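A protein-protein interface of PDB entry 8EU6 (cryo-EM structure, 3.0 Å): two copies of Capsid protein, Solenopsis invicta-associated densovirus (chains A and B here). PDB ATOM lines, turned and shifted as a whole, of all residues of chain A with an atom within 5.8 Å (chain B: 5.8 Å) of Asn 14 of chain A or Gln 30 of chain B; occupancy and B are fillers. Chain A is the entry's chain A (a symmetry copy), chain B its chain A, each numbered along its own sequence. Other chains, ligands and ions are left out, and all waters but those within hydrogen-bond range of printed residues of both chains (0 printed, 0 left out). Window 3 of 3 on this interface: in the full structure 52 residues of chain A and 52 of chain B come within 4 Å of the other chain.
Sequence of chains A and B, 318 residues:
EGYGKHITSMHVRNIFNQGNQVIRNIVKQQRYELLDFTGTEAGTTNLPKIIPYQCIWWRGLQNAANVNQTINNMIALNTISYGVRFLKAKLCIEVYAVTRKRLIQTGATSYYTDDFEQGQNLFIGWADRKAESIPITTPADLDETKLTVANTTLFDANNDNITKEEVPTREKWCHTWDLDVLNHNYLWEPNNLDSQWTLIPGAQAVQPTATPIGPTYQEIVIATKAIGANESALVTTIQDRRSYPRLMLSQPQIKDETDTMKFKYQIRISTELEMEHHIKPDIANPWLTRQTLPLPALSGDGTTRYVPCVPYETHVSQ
Of the printed residues of chain B, Asn 14 of chain A touches Gln 30. Of the printed residues of chain B, Phe 16 of chain A touches Lys 28 (3.8 Å) and Gln 30 (3.9 Å). Of the printed residues of chain A, Lys 28 of chain B touches Ile 15, Phe 16 and Asn 17. Of chain A, only Asn 14, Ile 15 and Phe 16 come within 4 Å of Gln 30 of chain B. Tyr 32 of chain B touches none of the printed residues of chain A. Printed residues of chain A within 4 Å of Arg 268 of chain B: Arg 13 (3.1 Å). The nearest residue of chain B that does not touch Asn 14 of chain A is Arg 268 of chain B (4.9 Å).
The backbone NH (N) of Gln 29 of chain B lies within hydrogen-bond range of the side-chain hydroxyl (OG1) of Thr 271 of chain B (3.0 Å). The side-chain amide nitrogen (NE2) of Gln 30 of chain B lies close to the guanidinium group (NE) of Arg 268 of chain B.
No position is printed for both chains.
NZ of Lys 28 of chain B is in hydrogen-bond range of O of Ile 15 of chain A (2.6 Å). OE1 of Gln 30 of chain B lies close to OD1 of Asn 14 of chain A, 2.5 Å away. The guanidinium group (NH2) of Arg 268 of chain B sits at hydrogen-bond distance from the backbone carbonyl oxygen (O) of Arg 13 of chain A (3.1 Å).
Along chain A the printed residues that touch a printed residue of chain B span positions 13 to 17. Among the printed residues, no Asp or Glu carboxylate lies within 4 Å of a Lys or Arg side-chain nitrogen of the other chain.
Ile 15 of chain A touches Gln 30 of chain B (CG1 to OE1, 3.3 Å). Ile 15 of chain A touches Thr 271 of chain B. Phe 16 of chain A touches Lys 28 of chain B. Phe 16 of chain A touches Gln 30 of chain B. Lys 28 of chain B touches Asn 17 of chain A (NZ to N, 3.8 Å).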
ATOM      1  N   VAL A  12     -23.844 -25.566  -1.841  1.00  0.00           N
ATOM      2  CA  VAL A  12     -24.601 -24.846  -2.853  1.00  0.00           C
ATOM      3  C   VAL A  12     -25.703 -24.063  -2.159  1.00  0.00           C
ATOM      4  O   VAL A  12     -26.532 -24.632  -1.439  1.00  0.00           O
ATOM      5  CB  VAL A  12     -25.173 -25.808  -3.898  1.00  0.00           C
ATOM      6  CG1 VAL A  12     -26.149 -26.778  -3.263  1.00  0.00           C
ATOM      7  CG2 VAL A  12     -25.837 -25.040  -4.997  1.00  0.00           C
ATOM      8  N   ARG A  13     -25.703 -22.749  -2.351  1.00  0.00           N
ATOM      9  CA  ARG A  13     -26.797 -21.932  -1.863  1.00  0.00           C
ATOM     10  C   ARG A  13     -26.952 -20.717  -2.751  1.00  0.00           C
ATOM     11  O   ARG A  13     -25.965 -20.121  -3.187  1.00  0.00           O
ATOM     12  CB  ARG A  13     -26.579 -21.479  -0.421  1.00  0.00           C
ATOM     13  CG  ARG A  13     -25.390 -20.568  -0.218  1.00  0.00           C
ATOM     14  CD  ARG A  13     -25.242 -20.202   1.252  1.00  0.00           C
ATOM     15  NE  ARG A  13     -26.230 -19.248   1.742  1.00  0.00           N
ATOM     16  CZ  ARG A  13     -26.439 -19.011   3.032  1.00  0.00           C
ATOM     17  NH1 ARG A  13     -25.758 -19.683   3.950  1.00  0.00           N
ATOM     18  NH2 ARG A  13     -27.342 -18.123   3.412  1.00  0.00           N
ATOM     19  N   ASN A  14     -28.201 -20.359  -3.010  1.00  0.00           N
ATOM     20  CA  ASN A  14     -28.544 -19.036  -3.492  1.00  0.00           C
ATOM     21  C   ASN A  14     -29.739 -18.592  -2.672  1.00  0.00           C
ATOM     22  O   ASN A  14     -30.824 -19.165  -2.793  1.00  0.00           O
ATOM     23  CB  ASN A  14     -28.850 -19.061  -4.985  1.00  0.00           C
ATOM     24  CG  ASN A  14     -28.799 -17.704  -5.611  1.00  0.00           C
ATOM     25  OD1 ASN A  14     -28.153 -16.793  -5.102  1.00  0.00           O
ATOM     26  ND2 ASN A  14     -29.423 -17.576  -6.767  1.00  0.00           N
ATOM     27  N   ILE A  15     -29.537 -17.573  -1.837  1.00  0.00           N
ATOM     28  CA  ILE A  15     -30.516 -17.238  -0.818  1.00  0.00           C
ATOM     29  C   ILE A  15     -31.836 -16.810  -1.424  1.00  0.00           C
ATOM     30  O   ILE A  15     -32.863 -16.807  -0.739  1.00  0.00           O
ATOM     31  CB  ILE A  15     -29.950 -16.145   0.092  1.00  0.00           C
ATOM     32  CG1 ILE A  15     -29.608 -14.915  -0.727  1.00  0.00           C
ATOM     33  CG2 ILE A  15     -28.718 -16.630   0.760  1.00  0.00           C
ATOM     34  CD1 ILE A  15     -29.219 -13.759   0.098  1.00  0.00           C
ATOM     35  N   PHE A  16     -31.830 -16.438  -2.693  1.00  0.00           N
ATOM     36  CA  PHE A  16     -33.032 -15.954  -3.340  1.00  0.00           C
ATOM     37  C   PHE A  16     -34.087 -17.051  -3.428  1.00  0.00           C
ATOM     38  O   PHE A  16     -33.779 -18.235  -3.581  1.00  0.00           O
ATOM     39  CB  PHE A  16     -32.670 -15.422  -4.714  1.00  0.00           C
ATOM     40  CG  PHE A  16     -31.781 -14.216  -4.679  1.00  0.00           C
ATOM     41  CD1 PHE A  16     -31.763 -13.379  -3.587  1.00  0.00           C
ATOM     42  CD2 PHE A  16     -30.936 -13.938  -5.727  1.00  0.00           C
ATOM     43  CE1 PHE A  16     -30.945 -12.282  -3.557  1.00  0.00           C
ATOM     44  CE2 PHE A  16     -30.115 -12.843  -5.691  1.00  0.00           C
ATOM     45  CZ  PHE A  16     -30.121 -12.018  -4.606  1.00  0.00           C
ATOM     46  N   ASN A  17     -35.347 -16.636  -3.325  1.00  0.00           N
ATOM     47  CA  ASN A  17     -36.466 -17.533  -3.078  1.00  0.00           C
ATOM     48  C   ASN A  17     -37.131 -18.055  -4.344  1.00  0.00           C
ATOM     49  O   ASN A  17     -37.962 -18.961  -4.258  1.00  0.00           O
ATOM     50  CB  ASN A  17     -37.514 -16.820  -2.218  1.00  0.00           C
ATOM     51  CG  ASN A  17     -38.311 -15.797  -2.998  1.00  0.00           C
ATOM     52  OD1 ASN A  17     -39.532 -15.713  -2.863  1.00  0.00           O
ATOM     53  ND2 ASN A  17     -37.629 -15.015  -3.821  1.00  0.00           N
ATOM     54  N   LYS B  28     -32.766  -9.498   1.080  1.00  0.00           N
ATOM     55  CA  LYS B  28     -31.675 -10.331   0.624  1.00  0.00           C
ATOM     56  C   LYS B  28     -30.808  -9.526  -0.318  1.00  0.00           C
ATOM     57  O   LYS B  28     -31.317  -8.844  -1.211  1.00  0.00           O
ATOM     58  CB  LYS B  28     -32.204 -11.582  -0.067  1.00  0.00           C
ATOM     59  CG  LYS B  28     -32.919 -12.513   0.866  1.00  0.00           C
ATOM     60  CD  LYS B  28     -33.553 -13.657   0.132  1.00  0.00           C
ATOM     61  CE  LYS B  28     -34.191 -14.623   1.084  1.00  0.00           C
ATOM     62  NZ  LYS B  28     -34.884 -15.706   0.367  1.00  0.00           N
ATOM     63  N   GLN B  29     -29.509  -9.575  -0.088  1.00  0.00           N
ATOM     64  CA  GLN B  29     -28.551  -8.935  -0.963  1.00  0.00           C
ATOM     65  C   GLN B  29     -27.349  -9.851  -1.055  1.00  0.00           C
ATOM     66  O   GLN B  29     -26.792 -10.254  -0.031  1.00  0.00           O
ATOM     67  CB  GLN B  29     -28.174  -7.557  -0.443  1.00  0.00           C
ATOM     68  CG  GLN B  29     -27.307  -6.794  -1.368  1.00  0.00           C
ATOM     69  CD  GLN B  29     -27.975  -6.525  -2.682  1.00  0.00           C
ATOM     70  OE1 GLN B  29     -27.762  -7.249  -3.647  1.00  0.00           O
ATOM     71  NE2 GLN B  29     -28.784  -5.480  -2.737  1.00  0.00           N
ATOM     72  N   GLN B  30     -26.959 -10.184  -2.276  1.00  0.00           N
ATOM     73  CA  GLN B  30     -25.963 -11.213  -2.507  1.00  0.00           C
ATOM     74  C   GLN B  30     -25.011 -10.716  -3.575  1.00  0.00           C
ATOM     75  O   GLN B  30     -25.447 -10.212  -4.613  1.00  0.00           O
ATOM     76  CB  GLN B  30     -26.630 -12.518  -2.927  1.00  0.00           C
ATOM     77  CG  GLN B  30     -25.718 -13.693  -2.980  1.00  0.00           C
ATOM     78  CD  GLN B  30     -26.457 -14.965  -3.283  1.00  0.00           C
ATOM     79  OE1 GLN B  30     -27.676 -14.966  -3.423  1.00  0.00           O
ATOM     80  NE2 GLN B  30     -25.730 -16.061  -3.363  1.00  0.00           N
ATOM     81  N   ARG B  31     -23.717 -10.854  -3.317  1.00  0.00           N
ATOM     82  CA  ARG B  31     -22.713 -10.193  -4.125  1.00  0.00           C
ATOM     83  C   ARG B  31     -21.458 -11.039  -4.169  1.00  0.00           C
ATOM     84  O   ARG B  31     -21.132 -11.729  -3.205  1.00  0.00           O
ATOM     85  CB  ARG B  31     -22.370  -8.826  -3.555  1.00  0.00           C
ATOM     86  CG  ARG B  31     -23.492  -7.845  -3.597  1.00  0.00           C
ATOM     87  CD  ARG B  31     -22.978  -6.481  -3.301  1.00  0.00           C
ATOM     88  NE  ARG B  31     -22.449  -6.428  -1.956  1.00  0.00           N
ATOM     89  CZ  ARG B  31     -23.200  -6.201  -0.893  1.00  0.00           C
ATOM     90  NH1 ARG B  31     -24.492  -6.019  -1.005  1.00  0.00           N
ATOM     91  NH2 ARG B  31     -22.656  -6.175   0.290  1.00  0.00           N
ATOM     92  N   TYR B  32     -20.755 -10.964  -5.291  1.00  0.00           N
ATOM     93  CA  TYR B  32     -19.426 -11.535  -5.451  1.00  0.00           C
ATOM     94  C   TYR B  32     -18.478 -10.364  -5.623  1.00  0.00           C
ATOM     95  O   TYR B  32     -18.501  -9.693  -6.659  1.00  0.00           O
ATOM     96  CB  TYR B  32     -19.367 -12.462  -6.655  1.00  0.00           C
ATOM     97  CG  TYR B  32     -18.002 -13.010  -6.971  1.00  0.00           C
ATOM     98  CD1 TYR B  32     -17.528 -14.145  -6.348  1.00  0.00           C
ATOM     99  CD2 TYR B  32     -17.184 -12.379  -7.883  1.00  0.00           C
ATOM    100  CE1 TYR B  32     -16.292 -14.652  -6.647  1.00  0.00           C
ATOM    101  CE2 TYR B  32     -15.946 -12.875  -8.184  1.00  0.00           C
ATOM    102  CZ  TYR B  32     -15.498 -14.008  -7.561  1.00  0.00           C
ATOM    103  OH  TYR B  32     -14.252 -14.500  -7.863  1.00  0.00           O
ATOM    104  N   ARG B 268     -18.082 -14.057  -1.864  1.00  0.00           N
ATOM    105  CA  ARG B 268     -19.498 -13.800  -2.055  1.00  0.00           C
ATOM    106  C   ARG B 268     -20.102 -13.549  -0.688  1.00  0.00           C
ATOM    107  O   ARG B 268     -20.133 -14.449   0.156  1.00  0.00           O
ATOM    108  CB  ARG B 268     -20.216 -14.947  -2.760  1.00  0.00           C
ATOM    109  CG  ARG B 268     -21.661 -14.637  -3.053  1.00  0.00           C
ATOM    110  CD  ARG B 268     -22.401 -15.745  -3.744  1.00  0.00           C
ATOM    111  NE  ARG B 268     -22.554 -16.929  -2.918  1.00  0.00           N
ATOM    112  CZ  ARG B 268     -23.040 -18.078  -3.366  1.00  0.00           C
ATOM    113  NH1 ARG B 268     -23.438 -18.186  -4.625  1.00  0.00           N
ATOM    114  NH2 ARG B 268     -23.147 -19.114  -2.551  1.00  0.00           N
ATOM    115  N   ILE B 269     -20.572 -12.332  -0.473  1.00  0.00           N
ATOM    116  CA  ILE B 269     -21.097 -11.909   0.812  1.00  0.00           C
ATOM    117  C   ILE B 269     -22.611 -11.970   0.728  1.00  0.00           C
ATOM    118  O   ILE B 269     -23.247 -11.168   0.036  1.00  0.00           O
ATOM    119  CB  ILE B 269     -20.602 -10.508   1.182  1.00  0.00           C
ATOM    120  CG1 ILE B 269     -21.053 -10.146   2.587  1.00  0.00           C
ATOM    121  CG2 ILE B 269     -21.115  -9.498   0.209  1.00  0.00           C
ATOM    122  CD1 ILE B 269     -20.390  -8.922   3.116  1.00  0.00           C
ATOM    123  N   SER B 270     -23.189 -12.930   1.433  1.00  0.00           N
ATOM    124  CA  SER B 270     -24.618 -13.178   1.399  1.00  0.00           C
ATOM    125  C   SER B 270     -25.256 -12.540   2.619  1.00  0.00           C
ATOM    126  O   SER B 270     -24.695 -12.583   3.717  1.00  0.00           O
ATOM    127  CB  SER B 270     -24.907 -14.676   1.367  1.00  0.00           C
ATOM    128  OG  SER B 270     -24.430 -15.281   0.180  1.00  0.00           O
ATOM    129  N   THR B 271     -26.426 -11.947   2.422  1.00  0.00           N
ATOM    130  CA  THR B 271     -27.104 -11.219   3.478  1.00  0.00           C
ATOM    131  C   THR B 271     -28.580 -11.559   3.486  1.00  0.00           C
ATOM    132  O   THR B 271     -29.222 -11.574   2.434  1.00  0.00           O
ATOM    133  CB  THR B 271     -26.937  -9.716   3.293  1.00  0.00           C
ATOM    134  OG1 THR B 271     -27.414  -9.329   2.001  1.00  0.00           O
ATOM    135  CG2 THR B 271     -25.499  -9.313   3.446  1.00  0.00           C
